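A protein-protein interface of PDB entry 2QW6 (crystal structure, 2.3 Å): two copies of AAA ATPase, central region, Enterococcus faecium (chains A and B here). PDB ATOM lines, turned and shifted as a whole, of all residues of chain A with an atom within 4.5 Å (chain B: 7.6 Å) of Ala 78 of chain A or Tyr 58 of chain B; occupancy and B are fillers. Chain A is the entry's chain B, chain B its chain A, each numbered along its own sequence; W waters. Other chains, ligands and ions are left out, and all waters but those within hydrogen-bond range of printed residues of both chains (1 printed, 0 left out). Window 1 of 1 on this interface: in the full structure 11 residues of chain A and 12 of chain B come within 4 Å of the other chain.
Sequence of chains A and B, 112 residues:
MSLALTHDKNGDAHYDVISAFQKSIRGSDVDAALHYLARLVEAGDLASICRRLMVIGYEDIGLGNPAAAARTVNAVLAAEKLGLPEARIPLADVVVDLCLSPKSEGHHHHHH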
ATOM      1  N   ASN A  74     -22.002 -18.092 -19.412  1.00  0.00           N
ATOM      2  CA  ASN A  74     -23.422 -18.421 -19.227  1.00  0.00           C
ATOM      3  C   ASN A  74     -23.722 -19.911 -19.417  1.00  0.00           C
ATOM      4  O   ASN A  74     -24.464 -20.512 -18.624  1.00  0.00           O
ATOM      5  CB  ASN A  74     -24.297 -17.593 -20.174  1.00  0.00           C
ATOM      6  CG  ASN A  74     -24.116 -16.096 -19.967  1.00  0.00           C
ATOM      7  OD1 ASN A  74     -22.992 -15.574 -20.090  1.00  0.00           O
ATOM      8  ND2 ASN A  74     -25.209 -15.400 -19.633  1.00  0.00           N
ATOM      9  N   ALA A  75     -23.139 -20.493 -20.468  1.00  0.00           N
ATOM     10  CA  ALA A  75     -23.302 -21.920 -20.807  1.00  0.00           C
ATOM     11  C   ALA A  75     -22.711 -22.860 -19.760  1.00  0.00           C
ATOM     12  O   ALA A  75     -23.283 -23.910 -19.447  1.00  0.00           O
ATOM     13  CB  ALA A  75     -22.670 -22.198 -22.171  1.00  0.00           C
ATOM     14  N   VAL A  76     -21.557 -22.475 -19.221  1.00  0.00           N
ATOM     15  CA  VAL A  76     -20.932 -23.204 -18.093  1.00  0.00           C
ATOM     16  C   VAL A  76     -21.746 -23.134 -16.799  1.00  0.00           C
ATOM     17  O   VAL A  76     -21.909 -24.152 -16.124  1.00  0.00           O
ATOM     18  CB  VAL A  76     -19.457 -22.732 -17.882  1.00  0.00           C
ATOM     19  CG1 VAL A  76     -18.904 -23.105 -16.495  1.00  0.00           C
ATOM     20  CG2 VAL A  76     -18.583 -23.280 -18.974  1.00  0.00           C
ATOM     21  N   LEU A  77     -22.231 -21.948 -16.420  1.00  0.00           N
ATOM     22  CA  LEU A  77     -23.193 -21.853 -15.270  1.00  0.00           C
ATOM     23  C   LEU A  77     -24.444 -22.726 -15.477  1.00  0.00           C
ATOM     24  O   LEU A  77     -24.891 -23.397 -14.556  1.00  0.00           O
ATOM     25  CB  LEU A  77     -23.634 -20.405 -14.993  1.00  0.00           C
ATOM     26  CG  LEU A  77     -22.506 -19.448 -14.600  1.00  0.00           C
ATOM     27  CD1 LEU A  77     -22.972 -18.005 -14.675  1.00  0.00           C
ATOM     28  CD2 LEU A  77     -21.941 -19.792 -13.213  1.00  0.00           C
ATOM     29  N   ALA A  78     -25.001 -22.691 -16.680  1.00  0.00           N
ATOM     30  CA  ALA A  78     -26.153 -23.537 -17.030  1.00  0.00           C
ATOM     31  C   ALA A  78     -25.778 -25.020 -16.914  1.00  0.00           C
ATOM     32  O   ALA A  78     -26.492 -25.801 -16.256  1.00  0.00           O
ATOM     33  CB  ALA A  78     -26.649 -23.212 -18.414  1.00  0.00           C
ATOM     34  N   ALA A  79     -24.624 -25.397 -17.470  1.00  0.00           N
ATOM     35  CA  ALA A  79     -24.146 -26.789 -17.353  1.00  0.00           C
ATOM     36  C   ALA A  79     -23.969 -27.174 -15.908  1.00  0.00           C
ATOM     37  O   ALA A  79     -24.379 -28.262 -15.501  1.00  0.00           O
ATOM     38  CB  ALA A  79     -22.831 -27.013 -18.148  1.00  0.00           C
ATOM     39  N   GLU A  80     -23.380 -26.282 -15.115  1.00  0.00           N
ATOM     40  CA  GLU A  80     -23.185 -26.564 -13.673  1.00  0.00           C
ATOM     41  C   GLU A  80     -24.482 -26.673 -12.865  1.00  0.00           C
ATOM     42  O   GLU A  80     -24.577 -27.522 -11.953  1.00  0.00           O
ATOM     43  CB  GLU A  80     -22.257 -25.536 -13.013  1.00  0.00           C
ATOM     44  CG  GLU A  80     -20.821 -25.677 -13.464  1.00  0.00           C
ATOM     45  CD  GLU A  80     -19.922 -24.581 -12.933  1.00  0.00           C
ATOM     46  OE1 GLU A  80     -20.427 -23.474 -12.601  1.00  0.00           O
ATOM     47  OE2 GLU A  80     -18.693 -24.833 -12.845  1.00  0.00           O
ATOM     48  N   LYS A  81     -25.470 -25.822 -13.191  1.00  0.00           N
ATOM     49  CA  LYS A  81     -26.775 -25.864 -12.515  1.00  0.00           C
ATOM     50  C   LYS A  81     -27.548 -27.100 -12.938  1.00  0.00           C
ATOM     51  O   LYS A  81     -28.219 -27.730 -12.129  1.00  0.00           O
ATOM     52  CB  LYS A  81     -27.586 -24.603 -12.816  1.00  0.00           C
ATOM     53  CG  LYS A  81     -27.013 -23.352 -12.174  1.00  0.00           C
ATOM     54  CD  LYS A  81     -27.848 -22.091 -12.480  1.00  0.00           C
ATOM     55  CE  LYS A  81     -27.287 -20.871 -11.783  1.00  0.00           C
ATOM     56  NZ  LYS A  81     -27.194 -21.078 -10.288  1.00  0.00           N
ATOM     57  N   LEU A  82     -27.468 -27.457 -14.211  1.00  0.00           N
ATOM     58  CA  LEU A  82     -28.161 -28.652 -14.679  1.00  0.00           C
ATOM     59  C   LEU A  82     -27.472 -29.914 -14.178  1.00  0.00           C
ATOM     60  O   LEU A  82     -28.132 -30.862 -13.711  1.00  0.00           O
ATOM     61  CB  LEU A  82     -28.250 -28.679 -16.204  1.00  0.00           C
ATOM     62  CG  LEU A  82     -29.142 -27.646 -16.883  1.00  0.00           C
ATOM     63  CD1 LEU A  82     -28.963 -27.797 -18.366  1.00  0.00           C
ATOM     64  CD2 LEU A  82     -30.605 -27.848 -16.455  1.00  0.00           C
ATOM     65  N   ILE A  89     -26.486 -30.308 -23.009  1.00  0.00           N
ATOM     66  CA  ILE A  89     -27.259 -29.408 -23.874  1.00  0.00           C
ATOM     67  C   ILE A  89     -26.591 -28.022 -24.016  1.00  0.00           C
ATOM     68  O   ILE A  89     -26.250 -27.633 -25.127  1.00  0.00           O
ATOM     69  CB  ILE A  89     -28.762 -29.392 -23.441  1.00  0.00           C
ATOM     70  CG1 ILE A  89     -29.421 -30.724 -23.821  1.00  0.00           C
ATOM     71  CG2 ILE A  89     -29.520 -28.278 -24.061  1.00  0.00           C
ATOM     72  CD1 ILE A  89     -30.739 -31.011 -23.080  1.00  0.00           C
ATOM     73  N   PRO A  90     -26.368 -27.284 -22.900  1.00  0.00           N
ATOM     74  CA  PRO A  90     -25.640 -26.022 -23.085  1.00  0.00           C
ATOM     75  C   PRO A  90     -24.238 -26.177 -23.668  1.00  0.00           C
ATOM     76  O   PRO A  90     -23.821 -25.357 -24.479  1.00  0.00           O
ATOM     77  CB  PRO A  90     -25.572 -25.435 -21.662  1.00  0.00           C
ATOM     78  CG  PRO A  90     -25.939 -26.546 -20.744  1.00  0.00           C
ATOM     79  CD  PRO A  90     -26.813 -27.463 -21.504  1.00  0.00           C
ATOM     80  N   ASP A  93     -24.276 -26.789 -27.441  1.00  0.00           N
ATOM     81  CA  ASP A  93     -24.537 -25.470 -27.993  1.00  0.00           C
ATOM     82  C   ASP A  93     -23.286 -24.597 -28.063  1.00  0.00           C
ATOM     83  O   ASP A  93     -22.993 -23.993 -29.097  1.00  0.00           O
ATOM     84  CB  ASP A  93     -25.556 -24.778 -27.100  1.00  0.00           C
ATOM     85  CG  ASP A  93     -26.511 -23.944 -27.873  1.00  0.00           C
ATOM     86  OD1 ASP A  93     -27.394 -24.574 -28.524  1.00  0.00           O
ATOM     87  OD2 ASP A  93     -26.364 -22.678 -27.825  1.00  0.00           O
ATOM     88  N   ARG B  51     -34.758 -25.078 -14.254  1.00  0.00           N
ATOM     89  CA  ARG B  51     -34.131 -26.186 -14.996  1.00  0.00           C
ATOM     90  C   ARG B  51     -34.710 -26.286 -16.400  1.00  0.00           C
ATOM     91  O   ARG B  51     -33.959 -26.311 -17.387  1.00  0.00           O
ATOM     92  CB  ARG B  51     -34.214 -27.535 -14.239  1.00  0.00           C
ATOM     93  CG  ARG B  51     -33.295 -27.633 -12.994  1.00  0.00           C
ATOM     94  CD  ARG B  51     -33.385 -29.038 -12.254  1.00  0.00           C
ATOM     95  NE  ARG B  51     -32.855 -30.096 -13.120  1.00  0.00           N
ATOM     96  CZ  ARG B  51     -31.582 -30.511 -13.139  1.00  0.00           C
ATOM     97  NH1 ARG B  51     -30.694 -30.009 -12.287  1.00  0.00           N
ATOM     98  NH2 ARG B  51     -31.204 -31.444 -14.012  1.00  0.00           N
ATOM     99  N   ARG B  52     -36.035 -26.267 -16.505  1.00  0.00           N
ATOM    100  CA  ARG B  52     -36.689 -26.438 -17.811  1.00  0.00           C
ATOM    101  C   ARG B  52     -36.387 -25.284 -18.771  1.00  0.00           C
ATOM    102  O   ARG B  52     -36.128 -25.500 -19.958  1.00  0.00           O
ATOM    103  CB  ARG B  52     -38.217 -26.593 -17.639  1.00  0.00           C
ATOM    104  CG  ARG B  52     -38.811 -27.867 -18.219  1.00  0.00           C
ATOM    105  CD  ARG B  52     -38.273 -29.114 -17.549  1.00  0.00           C
ATOM    106  NE  ARG B  52     -37.433 -29.888 -18.450  1.00  0.00           N
ATOM    107  CZ  ARG B  52     -36.167 -30.283 -18.212  1.00  0.00           C
ATOM    108  NH1 ARG B  52     -35.535 -29.984 -17.065  1.00  0.00           N
ATOM    109  NH2 ARG B  52     -35.524 -30.995 -19.142  1.00  0.00           N
ATOM    110  N   LEU B  53     -36.408 -24.058 -18.245  1.00  0.00           N
ATOM    111  CA  LEU B  53     -36.126 -22.873 -19.051  1.00  0.00           C
ATOM    112  C   LEU B  53     -34.726 -22.898 -19.655  1.00  0.00           C
ATOM    113  O   LEU B  53     -34.557 -22.512 -20.811  1.00  0.00           O
ATOM    114  CB  LEU B  53     -36.308 -21.592 -18.251  1.00  0.00           C
ATOM    115  CG  LEU B  53     -37.766 -21.158 -17.987  1.00  0.00           C
ATOM    116  CD1 LEU B  53     -37.784 -19.883 -17.126  1.00  0.00           C
ATOM    117  CD2 LEU B  53     -38.578 -20.939 -19.271  1.00  0.00           C
ATOM    118  N   MET B  54     -33.736 -23.328 -18.876  1.00  0.00           N
ATOM    119  CA  MET B  54     -32.360 -23.398 -19.368  1.00  0.00           C
ATOM    120  C   MET B  54     -32.211 -24.470 -20.453  1.00  0.00           C
ATOM    121  O   MET B  54     -31.523 -24.253 -21.465  1.00  0.00           O
ATOM    122  CB  MET B  54     -31.354 -23.599 -18.215  1.00  0.00           C
ATOM    123  CG  MET B  54     -31.030 -22.268 -17.468  1.00  0.00           C
ATOM    124  SD  MET B  54     -29.797 -22.332 -16.132  1.00  0.00           S
ATOM    125  CE  MET B  54     -30.417 -23.640 -15.099  1.00  0.00           C
ATOM    126  N   VAL B  55     -32.853 -25.616 -20.244  1.00  0.00           N
ATOM    127  CA  VAL B  55     -32.839 -26.673 -21.261  1.00  0.00           C
ATOM    128  C   VAL B  55     -33.470 -26.207 -22.588  1.00  0.00           C
ATOM    129  O   VAL B  55     -32.845 -26.273 -23.636  1.00  0.00           O
ATOM    130  CB  VAL B  55     -33.450 -27.999 -20.753  1.00  0.00           C
ATOM    131  CG1 VAL B  55     -33.614 -29.019 -21.915  1.00  0.00           C
ATOM    132  CG2 VAL B  55     -32.554 -28.588 -19.693  1.00  0.00           C
ATOM    133  N   ILE B  56     -34.686 -25.700 -22.520  1.00  0.00           N
ATOM    134  CA  ILE B  56     -35.337 -25.133 -23.677  1.00  0.00           C
ATOM    135  C   ILE B  56     -34.513 -24.031 -24.318  1.00  0.00           C
ATOM    136  O   ILE B  56     -34.383 -23.987 -25.540  1.00  0.00           O
ATOM    137  CB  ILE B  56     -36.727 -24.570 -23.307  1.00  0.00           C
ATOM    138  CG1 ILE B  56     -37.677 -25.706 -22.896  1.00  0.00           C
ATOM    139  CG2 ILE B  56     -37.300 -23.769 -24.483  1.00  0.00           C
ATOM    140  CD1 ILE B  56     -38.825 -25.216 -22.017  1.00  0.00           C
ATOM    141  N   GLY B  57     -33.973 -23.120 -23.515  1.00  0.00           N
ATOM    142  CA  GLY B  57     -33.163 -22.047 -24.081  1.00  0.00           C
ATOM    143  C   GLY B  57     -32.019 -22.612 -24.916  1.00  0.00           C
ATOM    144  O   GLY B  57     -31.784 -22.148 -26.014  1.00  0.00           O
ATOM    145  N   TYR B  58     -31.315 -23.619 -24.402  1.00  0.00           N
ATOM    146  CA  TYR B  58     -30.110 -24.118 -25.065  1.00  0.00           C
ATOM    147  C   TYR B  58     -30.400 -25.174 -26.118  1.00  0.00           C
ATOM    148  O   TYR B  58     -29.624 -25.324 -27.044  1.00  0.00           O
ATOM    149  CB  TYR B  58     -29.031 -24.603 -24.053  1.00  0.00           C
ATOM    150  CG  TYR B  58     -28.223 -23.446 -23.465  1.00  0.00           C
ATOM    151  CD1 TYR B  58     -27.222 -22.816 -24.207  1.00  0.00           C
ATOM    152  CD2 TYR B  58     -28.516 -22.943 -22.186  1.00  0.00           C
ATOM    153  CE1 TYR B  58     -26.507 -21.725 -23.683  1.00  0.00           C
ATOM    154  CE2 TYR B  58     -27.808 -21.857 -21.652  1.00  0.00           C
ATOM    155  CZ  TYR B  58     -26.804 -21.255 -22.398  1.00  0.00           C
ATOM    156  OH  TYR B  58     -26.115 -20.186 -21.859  1.00  0.00           O
ATOM    157  N   GLU B  59     -31.514 -25.888 -25.975  1.00  0.00           N
ATOM    158  CA  GLU B  59     -31.872 -26.962 -26.893  1.00  0.00           C
ATOM    159  C   GLU B  59     -32.711 -26.458 -28.065  1.00  0.00           C
ATOM    160  O   GLU B  59     -32.357 -26.671 -29.226  1.00  0.00           O
ATOM    161  CB  GLU B  59     -32.619 -28.091 -26.172  1.00  0.00           C
ATOM    162  CG  GLU B  59     -33.001 -29.225 -27.126  1.00  0.00           C
ATOM    163  CD  GLU B  59     -33.552 -30.463 -26.442  1.00  0.00           C
ATOM    164  OE1 GLU B  59     -33.866 -30.391 -25.228  1.00  0.00           O
ATOM    165  OE2 GLU B  59     -33.691 -31.506 -27.140  1.00  0.00           O
ATOM    166  N   ASP B  60     -33.823 -25.790 -27.748  1.00  0.00           N
ATOM    167  CA  ASP B  60     -34.788 -25.374 -28.756  1.00  0.00           C
ATOM    168  C   ASP B  60     -34.447 -24.033 -29.388  1.00  0.00           C
ATOM    169  O   ASP B  60     -35.032 -23.664 -30.395  1.00  0.00           O
ATOM    170  CB  ASP B  60     -36.201 -25.380 -28.169  1.00  0.00           C
ATOM    171  CG  ASP B  60     -36.550 -26.712 -27.539  1.00  0.00           C
ATOM    172  OD1 ASP B  60     -36.433 -27.744 -28.235  1.00  0.00           O
ATOM    173  OD2 ASP B  60     -36.916 -26.738 -26.345  1.00  0.00           O
ATOM    174  N   ILE B  61     -33.474 -23.335 -28.804  1.00  0.00           N
ATOM    175  CA  ILE B  61     -33.012 -22.013 -29.247  1.00  0.00           C
ATOM    176  C   ILE B  61     -31.480 -22.032 -29.056  1.00  0.00           C
ATOM    177  O   ILE B  61     -30.711 -21.302 -29.698  1.00  0.00           O
ATOM    178  CB  ILE B  61     -33.691 -20.891 -28.367  1.00  0.00           C
ATOM    179  CG1 ILE B  61     -35.169 -21.269 -28.087  1.00  0.00           C
ATOM    180  CG2 ILE B  61     -33.496 -19.513 -28.959  1.00  0.00           C
ATOM    181  CD1 ILE B  61     -36.086 -20.201 -27.570  1.00  0.00           C
ATOM    182  N   PRO B  66     -28.409 -17.208 -30.016  1.00  0.00           N
ATOM    183  CA  PRO B  66     -27.532 -17.630 -28.916  1.00  0.00           C
ATOM    184  C   PRO B  66     -27.510 -16.639 -27.731  1.00  0.00           C
ATOM    185  O   PRO B  66     -27.176 -17.029 -26.596  1.00  0.00           O
ATOM    186  CB  PRO B  66     -26.149 -17.739 -29.583  1.00  0.00           C
ATOM    187  CG  PRO B  66     -26.208 -16.809 -30.751  1.00  0.00           C
ATOM    188  CD  PRO B  66     -27.647 -16.736 -31.195  1.00  0.00           C
ATOM    189  N   ALA B  67     -27.864 -15.383 -28.007  1.00  0.00           N
ATOM    190  CA  ALA B  67     -28.023 -14.359 -26.976  1.00  0.00           C
ATOM    191  C   ALA B  67     -29.252 -14.668 -26.148  1.00  0.00           C
ATOM    192  O   ALA B  67     -29.225 -14.517 -24.911  1.00  0.00           O
ATOM    193  CB  ALA B  67     -28.137 -12.975 -27.585  1.00  0.00           C
ATOM    194  N   ALA B  68     -30.317 -15.115 -26.812  1.00  0.00           N
ATOM    195  CA  ALA B  68     -31.513 -15.527 -26.100  1.00  0.00           C
ATOM    196  C   ALA B  68     -31.225 -16.738 -25.234  1.00  0.00           C
ATOM    197  O   ALA B  68     -31.737 -16.833 -24.115  1.00  0.00           O
ATOM    198  CB  ALA B  68     -32.642 -15.821 -27.045  1.00  0.00           C
ATOM    199  N   ALA B  69     -30.411 -17.662 -25.731  1.00  0.00           N
ATOM    200  CA  ALA B  69     -29.997 -18.812 -24.906  1.00  0.00           C
ATOM    201  C   ALA B  69     -29.269 -18.357 -23.621  1.00  0.00           C
ATOM    202  O   ALA B  69     -29.640 -18.747 -22.529  1.00  0.00           O
ATOM    203  CB  ALA B  69     -29.145 -19.790 -25.717  1.00  0.00           C
ATOM    204  N   ALA B  70     -28.267 -17.500 -23.777  1.00  0.00           N
ATOM    205  CA  ALA B  70     -27.487 -16.979 -22.657  1.00  0.00           C
ATOM    206  C   ALA B  70     -28.336 -16.200 -21.653  1.00  0.00           C
ATOM    207  O   ALA B  70     -28.132 -16.329 -20.442  1.00  0.00           O
ATOM    208  CB  ALA B  70     -26.323 -16.124 -23.155  1.00  0.00           C
ATOM    209  N   ARG B  71     -29.295 -15.426 -22.160  1.00  0.00           N
ATOM    210  CA  ARG B  71     -30.146 -14.588 -21.321  1.00  0.00           C
ATOM    211  C   ARG B  71     -31.095 -15.349 -20.397  1.00  0.00           C
ATOM    212  O   ARG B  71     -31.658 -14.773 -19.443  1.00  0.00           O
ATOM    213  CB  ARG B  71     -30.961 -13.629 -22.165  1.00  0.00           C
ATOM    214  CG  ARG B  71     -30.197 -12.441 -22.634  1.00  0.00           C
ATOM    215  CD  ARG B  71     -31.165 -11.378 -23.038  1.00  0.00           C
ATOM    216  NE  ARG B  71     -32.125 -11.869 -24.037  1.00  0.00           N
ATOM    217  CZ  ARG B  71     -31.992 -11.699 -25.354  1.00  0.00           C
ATOM    218  NH1 ARG B  71     -30.927 -11.060 -25.856  1.00  0.00           N
ATOM    219  NH2 ARG B  71     -32.922 -12.182 -26.167  1.00  0.00           N
ATOM    220  N   THR B  72     -31.286 -16.635 -20.663  1.00  0.00           N
ATOM    221  CA  THR B  72     -32.072 -17.456 -19.746  1.00  0.00           C
ATOM    222  C   THR B  72     -31.281 -17.690 -18.470  1.00  0.00           C
ATOM    223  O   THR B  72     -31.853 -17.821 -17.386  1.00  0.00           O
ATOM    224  CB  THR B  72     -32.459 -18.788 -20.393  1.00  0.00           C
ATOM    225  OG1 THR B  72     -32.940 -18.523 -21.716  1.00  0.00           O
ATOM    226  CG2 THR B  72     -33.574 -19.440 -19.616  1.00  0.00           C
ATOM    227  N   VAL B  73     -29.959 -17.732 -18.595  1.00  0.00           N
ATOM    228  CA  VAL B  73     -29.124 -17.880 -17.420  1.00  0.00           C
ATOM    229  C   VAL B  73     -29.270 -16.643 -16.501  1.00  0.00           C
ATOM    230  O   VAL B  73     -29.558 -16.791 -15.305  1.00  0.00           O
ATOM    231  CB  VAL B  73     -27.667 -18.258 -17.816  1.00  0.00           C
ATOM    232  CG1 VAL B  73     -26.812 -18.615 -16.595  1.00  0.00           C
ATOM    233  CG2 VAL B  73     -27.707 -19.447 -18.786  1.00  0.00           C
ATOM    234  N   ASN B  74     -29.134 -15.437 -17.063  1.00  0.00           N
ATOM    235  CA  ASN B  74     -29.346 -14.191 -16.283  1.00  0.00           C
ATOM    236  C   ASN B  74     -30.701 -14.194 -15.573  1.00  0.00           C
ATOM    237  O   ASN B  74     -30.779 -14.026 -14.355  1.00  0.00           O
ATOM    238  CB  ASN B  74     -29.214 -12.928 -17.150  1.00  0.00           C
ATOM    239  CG  ASN B  74     -27.883 -12.825 -17.828  1.00  0.00           C
ATOM    240  OD1 ASN B  74     -27.561 -13.619 -18.718  1.00  0.00           O
ATOM    241  ND2 ASN B  74     -27.091 -11.844 -17.421  1.00  0.00           N
ATOM    242  N   VAL B  76     -32.550 -16.702 -14.725  1.00  0.00           N
ATOM    243  CA  VAL B  76     -32.561 -17.755 -13.686  1.00  0.00           C
ATOM    244  C   VAL B  76     -31.775 -17.304 -12.455  1.00  0.00           C
ATOM    245  O   VAL B  76     -32.196 -17.509 -11.296  1.00  0.00           O
ATOM    246  CB  VAL B  76     -32.051 -19.147 -14.256  1.00  0.00           C
ATOM    247  CG1 VAL B  76     -31.683 -20.141 -13.157  1.00  0.00           C
ATOM    248  CG2 VAL B  76     -33.095 -19.772 -15.152  1.00  0.00           C
ATOM    249  N   LEU B  98     -38.685 -16.615 -24.899  1.00  0.00           N
ATOM    250  CA  LEU B  98     -38.446 -17.921 -25.532  1.00  0.00           C
ATOM    251  C   LEU B  98     -39.571 -18.372 -26.453  1.00  0.00           C
ATOM    252  O   LEU B  98     -39.324 -19.014 -27.496  1.00  0.00           O
ATOM    253  CB  LEU B  98     -38.193 -19.006 -24.474  1.00  0.00           C
ATOM    254  CG  LEU B  98     -36.930 -18.969 -23.595  1.00  0.00           C
ATOM    255  CD1 LEU B  98     -36.872 -20.239 -22.745  1.00  0.00           C
ATOM    256  CD2 LEU B  98     -35.652 -18.830 -24.405  1.00  0.00           C
HETATM  257  O   HOH W   1     -29.080 -33.457 -15.404  1.00  0.00           O
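The guanidinium group (NH1) of Arg 51 of chain B lies within hydrogen-bond range of the backbone carbonyl oxygen (O) of Lys 81 of chain A (3.4 Å). OD1 of Asn 74 of chain B is in hydrogen-bond range of ND2 of Asn 74 of chain A, at 3.1 Å. OD1 of Asp 93 of chain A lies close to O of Tyr 58 of chain B (2.8 Å). ND2 of Asn 74 of chain A sits at hydrogen-bond distance from O of Ala 70 of chain B, 3.2 Å away. OH of Tyr 58 of chain B lies within hydrogen-bond range of N of Ala 75 of chain A (3.3 Å). The guanidinium group (NH1) of Arg 51 of chain B lies within hydrogen-bond range of the backbone carbonyl oxygen (O) of Leu 82 of chain A (3.1 Å).
O of Ala 70 of chain B sits close to OD1 of Asn 74 of chain B (3.3 Å).
Among the printed residues, pairs that only touch across the chains: Asn 74 of chain A with Val 73 of chain B, Asn 74 of chain A with Tyr 58 of chain B, Ile 89 of chain A with Glu 59 of chain B, Pro 90 of chain A with Tyr 58 of chain B, Ile 89 of chain A with Val 55 of chain B, Ala 78 of chain A with Tyr 58 of chain B, Ile 89 of chain A with Tyr 58 of chain B, Lys 81 of chain A with Met 54 of chain B, Leu 82 of chain A with Val 55 of chain B, Ala 78 of chain A with Val 73 of chain B, Ala 78 of chain A with Met 54 of chain B and Leu 77 of chain A with Val 73 of chain B.
Of chain B, only Met 54 (3.9 Å), Tyr 58 (3.7 Å) and Val 73 (3.9 Å) come within 4 Å of Ala 78 of chain A. Of the printed residues of chain B, Leu 82 of chain A touches Arg 51 (3.1 Å) and Val 55 (3.9 Å). Of the printed residues of chain B, Ile 89 of chain A touches Val 55, Tyr 58 and Glu 59. Printed residues of chain B within 4 Å of Asp 93 of chain A: Tyr 58 (2.8 Å). Of chain A, only Asn 74, Ala 75, Ala 78, Ile 89, Pro 90 and Asp 93 come within 4 Å of Tyr 58 of chain B. Ala 69 of chain B touches none of the printed residues of chain A. Of the printed residues of chain A, Ala 70 of chain B touches Asn 74 (3.2 Å). The nearest residue of chain B that does not touch Ala 78 of chain A is Ala 69 of chain B (6.8 Å).
Hydrophobic or aromatic side chains of chain B within 4 Å of the printed part of chain A: Met 54, Val 55, Tyr 58, Ala 70 and Val 73.
Asn 74 of chain B touches its own counterpart, Asn 74 of chain A. Of the 18 pairs that touch across the chains among the printed residues, 1 has its exchanged pair printed and touching as well.
Water W1 bridges the backbone carbonyl oxygen (O) of Leu 82 of chain A and the guanidinium group (NH2) of Arg 51 of chain B.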
